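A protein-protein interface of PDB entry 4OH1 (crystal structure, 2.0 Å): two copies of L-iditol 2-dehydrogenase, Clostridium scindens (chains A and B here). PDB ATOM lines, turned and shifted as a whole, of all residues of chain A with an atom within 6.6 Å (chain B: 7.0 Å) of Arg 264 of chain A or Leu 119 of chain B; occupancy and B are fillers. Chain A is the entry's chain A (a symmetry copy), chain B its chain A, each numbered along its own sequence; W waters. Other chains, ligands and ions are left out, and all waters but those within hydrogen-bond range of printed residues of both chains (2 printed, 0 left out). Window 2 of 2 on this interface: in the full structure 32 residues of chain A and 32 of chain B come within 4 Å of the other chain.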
ATOM      1  N   ARG A 241       2.215  -0.051 -21.536  1.00  0.00           N
ATOM      2  CA  ARG A 241       1.362   0.635 -22.464  1.00  0.00           C
ATOM      3  C   ARG A 241       2.059   0.706 -23.851  1.00  0.00           C
ATOM      4  O   ARG A 241       3.239   0.376 -23.969  1.00  0.00           O
ATOM      5  CB  ARG A 241       0.976   1.981 -21.895  1.00  0.00           C
ATOM      6  CG  ARG A 241      -0.054   1.842 -20.829  1.00  0.00           C
ATOM      7  CD  ARG A 241      -0.684   3.139 -20.477  1.00  0.00           C
ATOM      8  NE  ARG A 241       0.153   3.809 -19.517  1.00  0.00           N
ATOM      9  CZ  ARG A 241       0.167   5.125 -19.299  1.00  0.00           C
ATOM     10  NH1 ARG A 241      -0.543   5.975 -20.034  1.00  0.00           N
ATOM     11  NH2 ARG A 241       0.959   5.598 -18.363  1.00  0.00           N
ATOM     12  N   TYR A 242       1.290   1.057 -24.880  1.00  0.00           N
ATOM     13  CA  TYR A 242       1.745   0.983 -26.245  1.00  0.00           C
ATOM     14  C   TYR A 242       2.443   2.230 -26.757  1.00  0.00           C
ATOM     15  O   TYR A 242       1.949   3.333 -26.601  1.00  0.00           O
ATOM     16  CB  TYR A 242       0.585   0.575 -27.152  1.00  0.00           C
ATOM     17  CG  TYR A 242       0.196  -0.858 -26.946  1.00  0.00           C
ATOM     18  CD1 TYR A 242      -0.591  -1.230 -25.864  1.00  0.00           C
ATOM     19  CD2 TYR A 242       0.599  -1.837 -27.810  1.00  0.00           C
ATOM     20  CE1 TYR A 242      -0.908  -2.549 -25.636  1.00  0.00           C
ATOM     21  CE2 TYR A 242       0.259  -3.197 -27.595  1.00  0.00           C
ATOM     22  CZ  TYR A 242      -0.469  -3.530 -26.510  1.00  0.00           C
ATOM     23  OH  TYR A 242      -0.841  -4.840 -26.288  1.00  0.00           O
ATOM     24  N   ASP A 243       3.588   2.059 -27.405  1.00  0.00           N
ATOM     25  CA  ASP A 243       4.302   3.253 -27.924  1.00  0.00           C
ATOM     26  C   ASP A 243       3.609   3.928 -29.120  1.00  0.00           C
ATOM     27  O   ASP A 243       3.704   5.130 -29.289  1.00  0.00           O
ATOM     28  CB  ASP A 243       5.743   2.941 -28.277  1.00  0.00           C
ATOM     29  CG  ASP A 243       6.483   2.242 -27.134  1.00  0.00           C
ATOM     30  OD1 ASP A 243       6.573   2.765 -26.014  1.00  0.00           O
ATOM     31  OD2 ASP A 243       6.957   1.139 -27.372  1.00  0.00           O
ATOM     32  N   LEU A 262      -2.234   4.198 -24.897  1.00  0.00           N
ATOM     33  CA  LEU A 262      -1.049   4.871 -25.289  1.00  0.00           C
ATOM     34  C   LEU A 262      -0.063   5.109 -24.106  1.00  0.00           C
ATOM     35  O   LEU A 262      -0.420   5.629 -23.074  1.00  0.00           O
ATOM     36  CB  LEU A 262      -1.456   6.206 -25.956  1.00  0.00           C
ATOM     37  CG  LEU A 262      -0.272   6.869 -26.700  1.00  0.00           C
ATOM     38  CD1 LEU A 262       0.156   6.097 -27.910  1.00  0.00           C
ATOM     39  CD2 LEU A 262      -0.700   8.284 -27.091  1.00  0.00           C
ATOM     40  N   ALA A 263       1.180   4.710 -24.289  1.00  0.00           N
ATOM     41  CA  ALA A 263       2.236   4.934 -23.296  1.00  0.00           C
ATOM     42  C   ALA A 263       2.597   6.386 -23.133  1.00  0.00           C
ATOM     43  O   ALA A 263       2.270   7.223 -23.974  1.00  0.00           O
ATOM     44  CB  ALA A 263       3.456   4.178 -23.690  1.00  0.00           C
ATOM     45  N   ARG A 264       3.295   6.692 -22.036  1.00  0.00           N
ATOM     46  CA  ARG A 264       3.824   8.019 -21.831  1.00  0.00           C
ATOM     47  C   ARG A 264       4.780   8.321 -22.967  1.00  0.00           C
ATOM     48  O   ARG A 264       5.517   7.453 -23.387  1.00  0.00           O
ATOM     49  CB  ARG A 264       4.537   8.144 -20.482  1.00  0.00           C
ATOM     50  CG  ARG A 264       3.642   7.884 -19.296  1.00  0.00           C
ATOM     51  CD  ARG A 264       4.407   8.008 -17.935  1.00  0.00           C
ATOM     52  NE  ARG A 264       4.471   9.397 -17.492  1.00  0.00           N
ATOM     53  CZ  ARG A 264       5.296   9.833 -16.544  1.00  0.00           C
ATOM     54  NH1 ARG A 264       6.132   8.988 -15.952  1.00  0.00           N
ATOM     55  NH2 ARG A 264       5.311  11.111 -16.179  1.00  0.00           N
ATOM     56  N   ASP A 265       4.738   9.537 -23.485  1.00  0.00           N
ATOM     57  CA  ASP A 265       5.499   9.900 -24.656  1.00  0.00           C
ATOM     58  C   ASP A 265       5.142   9.115 -25.943  1.00  0.00           C
ATOM     59  O   ASP A 265       5.897   9.137 -26.888  1.00  0.00           O
ATOM     60  CB  ASP A 265       7.016   9.776 -24.388  1.00  0.00           C
ATOM     61  CG  ASP A 265       7.843  10.649 -25.315  1.00  0.00           C
ATOM     62  OD1 ASP A 265       7.384  11.785 -25.646  1.00  0.00           O
ATOM     63  OD2 ASP A 265       8.960  10.232 -25.725  1.00  0.00           O
ATOM     64  N   GLY A 266       4.040   8.395 -25.968  1.00  0.00           N
ATOM     65  CA  GLY A 266       3.644   7.627 -27.137  1.00  0.00           C
ATOM     66  C   GLY A 266       2.982   8.464 -28.231  1.00  0.00           C
ATOM     67  O   GLY A 266       2.625   9.620 -27.997  1.00  0.00           O
ATOM     68  N   TYR A 289      -0.299  16.748 -19.808  1.00  0.00           N
ATOM     69  CA  TYR A 289       0.673  17.204 -18.848  1.00  0.00           C
ATOM     70  C   TYR A 289       1.430  16.016 -18.192  1.00  0.00           C
ATOM     71  O   TYR A 289       2.641  15.969 -18.311  1.00  0.00           O
ATOM     72  CB  TYR A 289       0.039  18.121 -17.820  1.00  0.00           C
ATOM     73  CG  TYR A 289       0.986  18.426 -16.705  1.00  0.00           C
ATOM     74  CD1 TYR A 289       2.040  19.317 -16.883  1.00  0.00           C
ATOM     75  CD2 TYR A 289       0.868  17.772 -15.490  1.00  0.00           C
ATOM     76  CE1 TYR A 289       2.893  19.570 -15.884  1.00  0.00           C
ATOM     77  CE2 TYR A 289       1.724  18.016 -14.476  1.00  0.00           C
ATOM     78  CZ  TYR A 289       2.734  18.905 -14.672  1.00  0.00           C
ATOM     79  OH  TYR A 289       3.576  19.124 -13.626  1.00  0.00           O
ATOM     80  N   TRP A 290       0.752  15.050 -17.571  1.00  0.00           N
ATOM     81  CA  TRP A 290       1.483  13.992 -16.847  1.00  0.00           C
ATOM     82  C   TRP A 290       2.061  12.994 -17.818  1.00  0.00           C
ATOM     83  O   TRP A 290       3.218  12.661 -17.695  1.00  0.00           O
ATOM     84  CB  TRP A 290       0.709  13.292 -15.680  1.00  0.00           C
ATOM     85  CG  TRP A 290       1.648  12.332 -14.921  1.00  0.00           C
ATOM     86  CD1 TRP A 290       1.679  10.986 -15.021  1.00  0.00           C
ATOM     87  CD2 TRP A 290       2.738  12.687 -14.051  1.00  0.00           C
ATOM     88  NE1 TRP A 290       2.687  10.470 -14.264  1.00  0.00           N
ATOM     89  CE2 TRP A 290       3.349  11.495 -13.648  1.00  0.00           C
ATOM     90  CE3 TRP A 290       3.233  13.897 -13.555  1.00  0.00           C
ATOM     91  CZ2 TRP A 290       4.439  11.473 -12.800  1.00  0.00           C
ATOM     92  CZ3 TRP A 290       4.303  13.870 -12.705  1.00  0.00           C
ATOM     93  CH2 TRP A 290       4.896  12.672 -12.339  1.00  0.00           C
ATOM     94  N   ASP A 291       1.296  12.559 -18.816  1.00  0.00           N
ATOM     95  CA  ASP A 291       1.745  11.492 -19.716  1.00  0.00           C
ATOM     96  C   ASP A 291       2.499  11.891 -21.010  1.00  0.00           C
ATOM     97  O   ASP A 291       3.075  11.039 -21.692  1.00  0.00           O
ATOM     98  CB  ASP A 291       0.567  10.537 -20.016  1.00  0.00           C
ATOM     99  CG  ASP A 291       0.303   9.578 -18.856  1.00  0.00           C
ATOM    100  OD1 ASP A 291       1.087   9.578 -17.869  1.00  0.00           O
ATOM    101  OD2 ASP A 291      -0.675   8.834 -18.954  1.00  0.00           O
ATOM    102  N   GLN A 292       2.520  13.174 -21.338  1.00  0.00           N
ATOM    103  CA  GLN A 292       3.261  13.616 -22.454  1.00  0.00           C
ATOM    104  C   GLN A 292       2.856  12.840 -23.744  1.00  0.00           C
ATOM    105  O   GLN A 292       3.689  12.435 -24.534  1.00  0.00           O
ATOM    106  CB  GLN A 292       4.772  13.495 -22.136  1.00  0.00           C
ATOM    107  CG  GLN A 292       5.600  14.370 -23.092  1.00  0.00           C
ATOM    108  CD  GLN A 292       7.054  14.539 -22.717  1.00  0.00           C
ATOM    109  OE1 GLN A 292       7.415  15.425 -21.933  1.00  0.00           O
ATOM    110  NE2 GLN A 292       7.909  13.691 -23.298  1.00  0.00           N
ATOM    111  N   LYS A 293       1.568  12.628 -23.935  1.00  0.00           N
ATOM    112  CA  LYS A 293       1.098  11.938 -25.119  1.00  0.00           C
ATOM    113  C   LYS A 293       1.153  12.839 -26.366  1.00  0.00           C
ATOM    114  O   LYS A 293       1.236  14.049 -26.271  1.00  0.00           O
ATOM    115  CB  LYS A 293      -0.284  11.344 -24.906  1.00  0.00           C
ATOM    116  CG  LYS A 293      -0.328  10.215 -23.883  1.00  0.00           C
ATOM    117  CD  LYS A 293      -1.763   9.895 -23.511  1.00  0.00           C
ATOM    118  CE  LYS A 293      -1.808   8.700 -22.551  1.00  0.00           C
ATOM    119  NZ  LYS A 293      -3.212   8.295 -22.367  1.00  0.00           N
ATOM    120  N   HIS A 294       1.264  12.209 -27.530  1.00  0.00           N
ATOM    121  CA  HIS A 294       1.271  12.926 -28.799  1.00  0.00           C
ATOM    122  C   HIS A 294       0.117  12.344 -29.591  1.00  0.00           C
ATOM    123  O   HIS A 294       0.060  11.116 -29.803  1.00  0.00           O
ATOM    124  CB  HIS A 294       2.590  12.777 -29.560  1.00  0.00           C
ATOM    125  CG  HIS A 294       3.796  12.962 -28.710  1.00  0.00           C
ATOM    126  ND1 HIS A 294       4.308  14.192 -28.414  1.00  0.00           N
ATOM    127  CD2 HIS A 294       4.579  12.068 -28.069  1.00  0.00           C
ATOM    128  CE1 HIS A 294       5.341  14.057 -27.599  1.00  0.00           C
ATOM    129  NE2 HIS A 294       5.518  12.780 -27.370  1.00  0.00           N
ATOM    130  N   TYR B 105      17.342  11.797 -11.036  1.00  0.00           N
ATOM    131  CA  TYR B 105      17.081  10.599 -11.819  1.00  0.00           C
ATOM    132  C   TYR B 105      17.792   9.381 -11.187  1.00  0.00           C
ATOM    133  O   TYR B 105      18.890   9.518 -10.670  1.00  0.00           O
ATOM    134  CB  TYR B 105      17.593  10.829 -13.245  1.00  0.00           C
ATOM    135  CG  TYR B 105      17.163  12.169 -13.785  1.00  0.00           C
ATOM    136  CD1 TYR B 105      15.813  12.539 -13.769  1.00  0.00           C
ATOM    137  CD2 TYR B 105      18.088  13.075 -14.287  1.00  0.00           C
ATOM    138  CE1 TYR B 105      15.391  13.783 -14.237  1.00  0.00           C
ATOM    139  CE2 TYR B 105      17.675  14.338 -14.778  1.00  0.00           C
ATOM    140  CZ  TYR B 105      16.317  14.672 -14.753  1.00  0.00           C
ATOM    141  OH  TYR B 105      15.849  15.880 -15.224  1.00  0.00           O
ATOM    142  N   CYS B 109      16.355   2.628 -13.881  1.00  0.00           N
ATOM    143  CA  CYS B 109      15.063   2.153 -14.387  1.00  0.00           C
ATOM    144  C   CYS B 109      15.033   2.217 -15.952  1.00  0.00           C
ATOM    145  O   CYS B 109      15.963   2.770 -16.629  1.00  0.00           O
ATOM    146  CB  CYS B 109      13.909   3.009 -13.800  1.00  0.00           C
ATOM    147  SG  CYS B 109      13.721   4.653 -14.601  1.00  0.00           S
ATOM    148  N   GLU B 110      13.961   1.673 -16.537  1.00  0.00           N
ATOM    149  CA  GLU B 110      13.913   1.536 -17.991  1.00  0.00           C
ATOM    150  C   GLU B 110      13.801   2.909 -18.655  1.00  0.00           C
ATOM    151  O   GLU B 110      14.511   3.194 -19.644  1.00  0.00           O
ATOM    152  CB  GLU B 110      12.785   0.632 -18.444  1.00  0.00           C
ATOM    153  CG  GLU B 110      12.781   0.511 -19.953  1.00  0.00           C
ATOM    154  CD  GLU B 110      11.820  -0.533 -20.470  1.00  0.00           C
ATOM    155  OE1 GLU B 110      12.167  -1.690 -20.289  1.00  0.00           O
ATOM    156  OE2 GLU B 110      10.742  -0.205 -21.058  1.00  0.00           O
ATOM    157  N   ASN B 111      12.949   3.779 -18.133  1.00  0.00           N
ATOM    158  CA  ASN B 111      12.897   5.099 -18.725  1.00  0.00           C
ATOM    159  C   ASN B 111      14.255   5.827 -18.693  1.00  0.00           C
ATOM    160  O   ASN B 111      14.683   6.486 -19.693  1.00  0.00           O
ATOM    161  CB  ASN B 111      11.804   5.912 -18.060  1.00  0.00           C
ATOM    162  CG  ASN B 111      10.418   5.438 -18.473  1.00  0.00           C
ATOM    163  OD1 ASN B 111      10.212   5.003 -19.583  1.00  0.00           O
ATOM    164  ND2 ASN B 111       9.492   5.499 -17.575  1.00  0.00           N
ATOM    165  N   CYS B 112      14.915   5.729 -17.539  1.00  0.00           N
ATOM    166  CA  CYS B 112      16.201   6.336 -17.376  1.00  0.00           C
ATOM    167  C   CYS B 112      17.100   5.784 -18.443  1.00  0.00           C
ATOM    168  O   CYS B 112      17.722   6.531 -19.134  1.00  0.00           O
ATOM    169  CB  CYS B 112      16.793   6.078 -15.973  1.00  0.00           C
ATOM    170  SG  CYS B 112      16.301   7.426 -14.836  1.00  0.00           S
ATOM    171  N   GLY B 115      16.957   7.004 -21.930  1.00  0.00           N
ATOM    172  CA  GLY B 115      17.241   8.418 -22.101  1.00  0.00           C
ATOM    173  C   GLY B 115      16.101   9.325 -21.660  1.00  0.00           C
ATOM    174  O   GLY B 115      16.222  10.583 -21.721  1.00  0.00           O
ATOM    175  N   LYS B 116      15.001   8.729 -21.182  1.00  0.00           N
ATOM    176  CA  LYS B 116      13.830   9.527 -20.892  1.00  0.00           C
ATOM    177  C   LYS B 116      13.782   9.795 -19.389  1.00  0.00           C
ATOM    178  O   LYS B 116      12.896   9.364 -18.684  1.00  0.00           O
ATOM    179  CB  LYS B 116      12.602   8.821 -21.419  1.00  0.00           C
ATOM    180  CG  LYS B 116      12.727   8.437 -22.904  1.00  0.00           C
ATOM    181  CD  LYS B 116      11.427   8.661 -23.673  1.00  0.00           C
ATOM    182  CE  LYS B 116      11.261   7.730 -24.857  1.00  0.00           C
ATOM    183  NZ  LYS B 116      10.934   6.397 -24.306  1.00  0.00           N
ATOM    184  N   VAL B 117      14.782  10.505 -18.904  1.00  0.00           N
ATOM    185  CA  VAL B 117      14.970  10.644 -17.464  1.00  0.00           C
ATOM    186  C   VAL B 117      13.843  11.478 -16.834  1.00  0.00           C
ATOM    187  O   VAL B 117      13.555  11.315 -15.674  1.00  0.00           O
ATOM    188  CB  VAL B 117      16.382  11.250 -17.112  1.00  0.00           C
ATOM    189  CG1 VAL B 117      17.542  10.240 -17.360  1.00  0.00           C
ATOM    190  CG2 VAL B 117      16.644  12.536 -17.863  1.00  0.00           C
ATOM    191  N   ASN B 118      13.222  12.377 -17.602  1.00  0.00           N
ATOM    192  CA  ASN B 118      12.027  13.096 -17.151  1.00  0.00           C
ATOM    193  C   ASN B 118      10.806  12.230 -16.889  1.00  0.00           C
ATOM    194  O   ASN B 118       9.841  12.720 -16.286  1.00  0.00           O
ATOM    195  CB  ASN B 118      11.656  14.178 -18.148  1.00  0.00           C
ATOM    196  CG  ASN B 118      11.268  13.601 -19.529  1.00  0.00           C
ATOM    197  OD1 ASN B 118      12.005  12.784 -20.112  1.00  0.00           O
ATOM    198  ND2 ASN B 118      10.076  13.988 -20.020  1.00  0.00           N
ATOM    199  N   LEU B 119      10.860  10.960 -17.333  1.00  0.00           N
ATOM    200  CA  LEU B 119       9.850   9.949 -17.040  1.00  0.00           C
ATOM    201  C   LEU B 119      10.415   8.944 -16.067  1.00  0.00           C
ATOM    202  O   LEU B 119       9.909   7.834 -15.971  1.00  0.00           O
ATOM    203  CB  LEU B 119       9.389   9.197 -18.333  1.00  0.00           C
ATOM    204  CG  LEU B 119       9.025  10.081 -19.530  1.00  0.00           C
ATOM    205  CD1 LEU B 119       8.744   9.224 -20.749  1.00  0.00           C
ATOM    206  CD2 LEU B 119       7.835  10.992 -19.182  1.00  0.00           C
ATOM    207  N   CYS B 120      11.467   9.300 -15.343  1.00  0.00           N
ATOM    208  CA  CYS B 120      12.091   8.345 -14.382  1.00  0.00           C
ATOM    209  C   CYS B 120      11.041   7.683 -13.472  1.00  0.00           C
ATOM    210  O   CYS B 120      10.236   8.382 -12.856  1.00  0.00           O
ATOM    211  CB  CYS B 120      13.198   9.024 -13.505  1.00  0.00           C
ATOM    212  SG  CYS B 120      13.756   7.939 -12.136  1.00  0.00           S
ATOM    213  N   SER B 121      11.075   6.354 -13.366  1.00  0.00           N
ATOM    214  CA  SER B 121      10.196   5.628 -12.393  1.00  0.00           C
ATOM    215  C   SER B 121      10.471   5.787 -10.917  1.00  0.00           C
ATOM    216  O   SER B 121       9.603   5.500 -10.128  1.00  0.00           O
ATOM    217  CB  SER B 121      10.285   4.118 -12.598  1.00  0.00           C
ATOM    218  OG  SER B 121       9.958   3.814 -13.904  1.00  0.00           O
ATOM    219  N   ASN B 122      11.708   6.080 -10.535  1.00  0.00           N
ATOM    220  CA  ASN B 122      12.054   6.288  -9.128  1.00  0.00           C
ATOM    221  C   ASN B 122      12.484   7.724  -8.912  1.00  0.00           C
ATOM    222  O   ASN B 122      13.484   8.011  -8.242  1.00  0.00           O
ATOM    223  CB  ASN B 122      13.185   5.378  -8.709  1.00  0.00           C
ATOM    224  CG  ASN B 122      12.900   3.957  -9.027  1.00  0.00           C
ATOM    225  OD1 ASN B 122      13.675   3.280  -9.685  1.00  0.00           O
ATOM    226  ND2 ASN B 122      11.738   3.513  -8.632  1.00  0.00           N
ATOM    227  N   MET B 123      11.702   8.618  -9.473  1.00  0.00           N
ATOM    228  CA  MET B 123      12.066  10.012  -9.519  1.00  0.00           C
ATOM    229  C   MET B 123      12.224  10.548  -8.098  1.00  0.00           C
ATOM    230  O   MET B 123      11.397  10.279  -7.267  1.00  0.00           O
ATOM    231  CB  MET B 123      10.970  10.770 -10.248  1.00  0.00           C
ATOM    232  CG  MET B 123      11.272  12.264 -10.381  1.00  0.00           C
ATOM    233  SD  MET B 123      12.617  12.617 -11.770  1.00  0.00           S
ATOM    234  CE  MET B 123      11.332  12.490 -13.279  1.00  0.00           C
ATOM    235  N   ILE B 299       6.113  17.118 -20.090  1.00  0.00           N
ATOM    236  CA  ILE B 299       6.506  17.025 -18.658  1.00  0.00           C
ATOM    237  C   ILE B 299       8.024  17.143 -18.362  1.00  0.00           C
ATOM    238  O   ILE B 299       8.850  16.294 -18.746  1.00  0.00           O
ATOM    239  CB  ILE B 299       5.939  15.768 -17.900  1.00  0.00           C
ATOM    240  CG1 ILE B 299       6.218  15.942 -16.360  1.00  0.00           C
ATOM    241  CG2 ILE B 299       6.467  14.443 -18.547  1.00  0.00           C
ATOM    242  CD1 ILE B 299       5.170  15.432 -15.348  1.00  0.00           C
ATOM    243  N   GLN B 300       8.335  18.235 -17.660  1.00  0.00           N
ATOM    244  CA  GLN B 300       9.647  18.546 -17.049  1.00  0.00           C
ATOM    245  C   GLN B 300      10.705  18.995 -18.032  1.00  0.00           C
ATOM    246  O   GLN B 300      11.404  19.958 -17.736  1.00  0.00           O
ATOM    247  CB  GLN B 300      10.212  17.400 -16.190  1.00  0.00           C
ATOM    248  CG  GLN B 300       9.510  17.192 -14.871  1.00  0.00           C
ATOM    249  CD  GLN B 300      10.209  16.155 -13.986  1.00  0.00           C
ATOM    250  OE1 GLN B 300      11.403  15.852 -14.158  1.00  0.00           O
ATOM    251  NE2 GLN B 300       9.458  15.601 -13.047  1.00  0.00           N
ATOM    252  N   GLY B 301      10.820  18.326 -19.177  1.00  0.00           N
ATOM    253  CA  GLY B 301      11.994  18.505 -20.040  1.00  0.00           C
ATOM    254  C   GLY B 301      13.102  17.515 -19.590  1.00  0.00           C
ATOM    255  O   GLY B 301      13.093  17.013 -18.436  1.00  0.00           O
ATOM    256  N   ALA B 302      14.032  17.215 -20.491  1.00  0.00           N
ATOM    257  CA  ALA B 302      15.132  16.293 -20.246  1.00  0.00           C
ATOM    258  C   ALA B 302      16.376  16.799 -20.912  1.00  0.00           C
ATOM    259  O   ALA B 302      16.303  17.180 -22.086  1.00  0.00           O
ATOM    260  CB  ALA B 302      14.833  14.939 -20.862  1.00  0.00           C
HETATM  261  O   HOH W   1       7.672  12.554 -14.619  1.00  0.00           O
HETATM  262  O   HOH W   2       8.233  10.038 -13.563  1.00  0.00           O
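ND2 of Asn 118 of chain B sits at hydrogen-bond distance from O of Ile 299 of chain B, 2.9 Å away. The guanidinium group of Arg 264 of chain A lies within salt-bridge range of the side-chain carboxylate of Asp 291 of chain A (3.4 Å). O of Asp 291 of chain A sits at hydrogen-bond distance from N of Asp 265 of chain A. OD1 of Asp 265 of chain A is in hydrogen-bond range of NE2 of Gln 292 of chain A (3.1 Å). The side-chain carboxylate (OD1) of Asp 265 of chain A sits at hydrogen-bond distance from a ring nitrogen (NE2) of His 294 of chain A (2.7 Å). NE2 of His 294 of chain A is in hydrogen-bond range of O of Gln 292 of chain A.
Printed residues of chain B within 4 Å of Arg 264 of chain A: Leu 119. Leu 119 of chain B touches just one residue of chain A: Arg 264 (3.8 Å). Of the printed residues of chain B, Gln 292 of chain A touches Asn 118 (3.6 Å) and Ile 299 (2.8 Å). Of the printed residues of chain B, Asp 265 of chain A touches Lys 116. Printed residues of chain A within 4 Å of Ile 299 of chain B: Tyr 289 (3.3 Å), Trp 290 (3.1 Å) and Gln 292 (2.8 Å). Printed residues of chain B within 4 Å of Trp 290 of chain A: Ile 299 (3.1 Å). Of the printed residues of chain B, Tyr 289 of chain A touches Ile 299 (3.3 Å). The nearest residue of chain B that does not touch Arg 264 of chain A is Ile 299 of chain B (4.2 Å). The nearest residue of chain A that does not touch Leu 119 of chain B is Asp 265 of chain A (4.1 Å).
Printed residues of chain A that touch a printed residue of chain B: Arg 264, Asp 265, Tyr 289, Trp 290 and Gln 292. Hydrophobic or aromatic side chains of chain A that line the printed part of chain B: Trp 290. Of the 18 printed residues of chain B, 4 touch a printed residue of chain A. Printed residues of chain B that touch a printed residue of chain A: Lys 116, Asn 118, Leu 119 and Ile 299. Among the printed residues, no Asp or Glu carboxylate lies within 4 Å of a Lys or Arg side-chain nitrogen of the other chain.
Among the printed residues, merely in contact across the chains: Trp 290 of chain A with Ile 299 of chain B (3.1 Å), Tyr 289 of chain A with Ile 299 of chain B (3.3 Å), Asp 265 of chain A with Lys 116 of chain B (3.5 Å), Gln 292 of chain A with Asn 118 of chain B (3.6 Å) and Arg 264 of chain A with Leu 119 of chain B (3.8 Å).
The backbone NH of Ile 299 of chain B lies within hydrogen-bond range of the side-chain amide oxygen of Gln 292 of chain A (2.8 Å).
Water W2 lies within hydrogen-bond range of O of Cys 120 of chain B (2.7 Å) and NH1 of Arg 264 of chain A (3.4 Å). Water W1 bridges the backbone carbonyl oxygen of Asn 118 of chain B and the guanidinium group of Arg 264 of chain A.
No position is printed for both chains. Of the 6 pairs that touch across the chains among the printed residues, none has its exchanged pair printed and touching as well.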
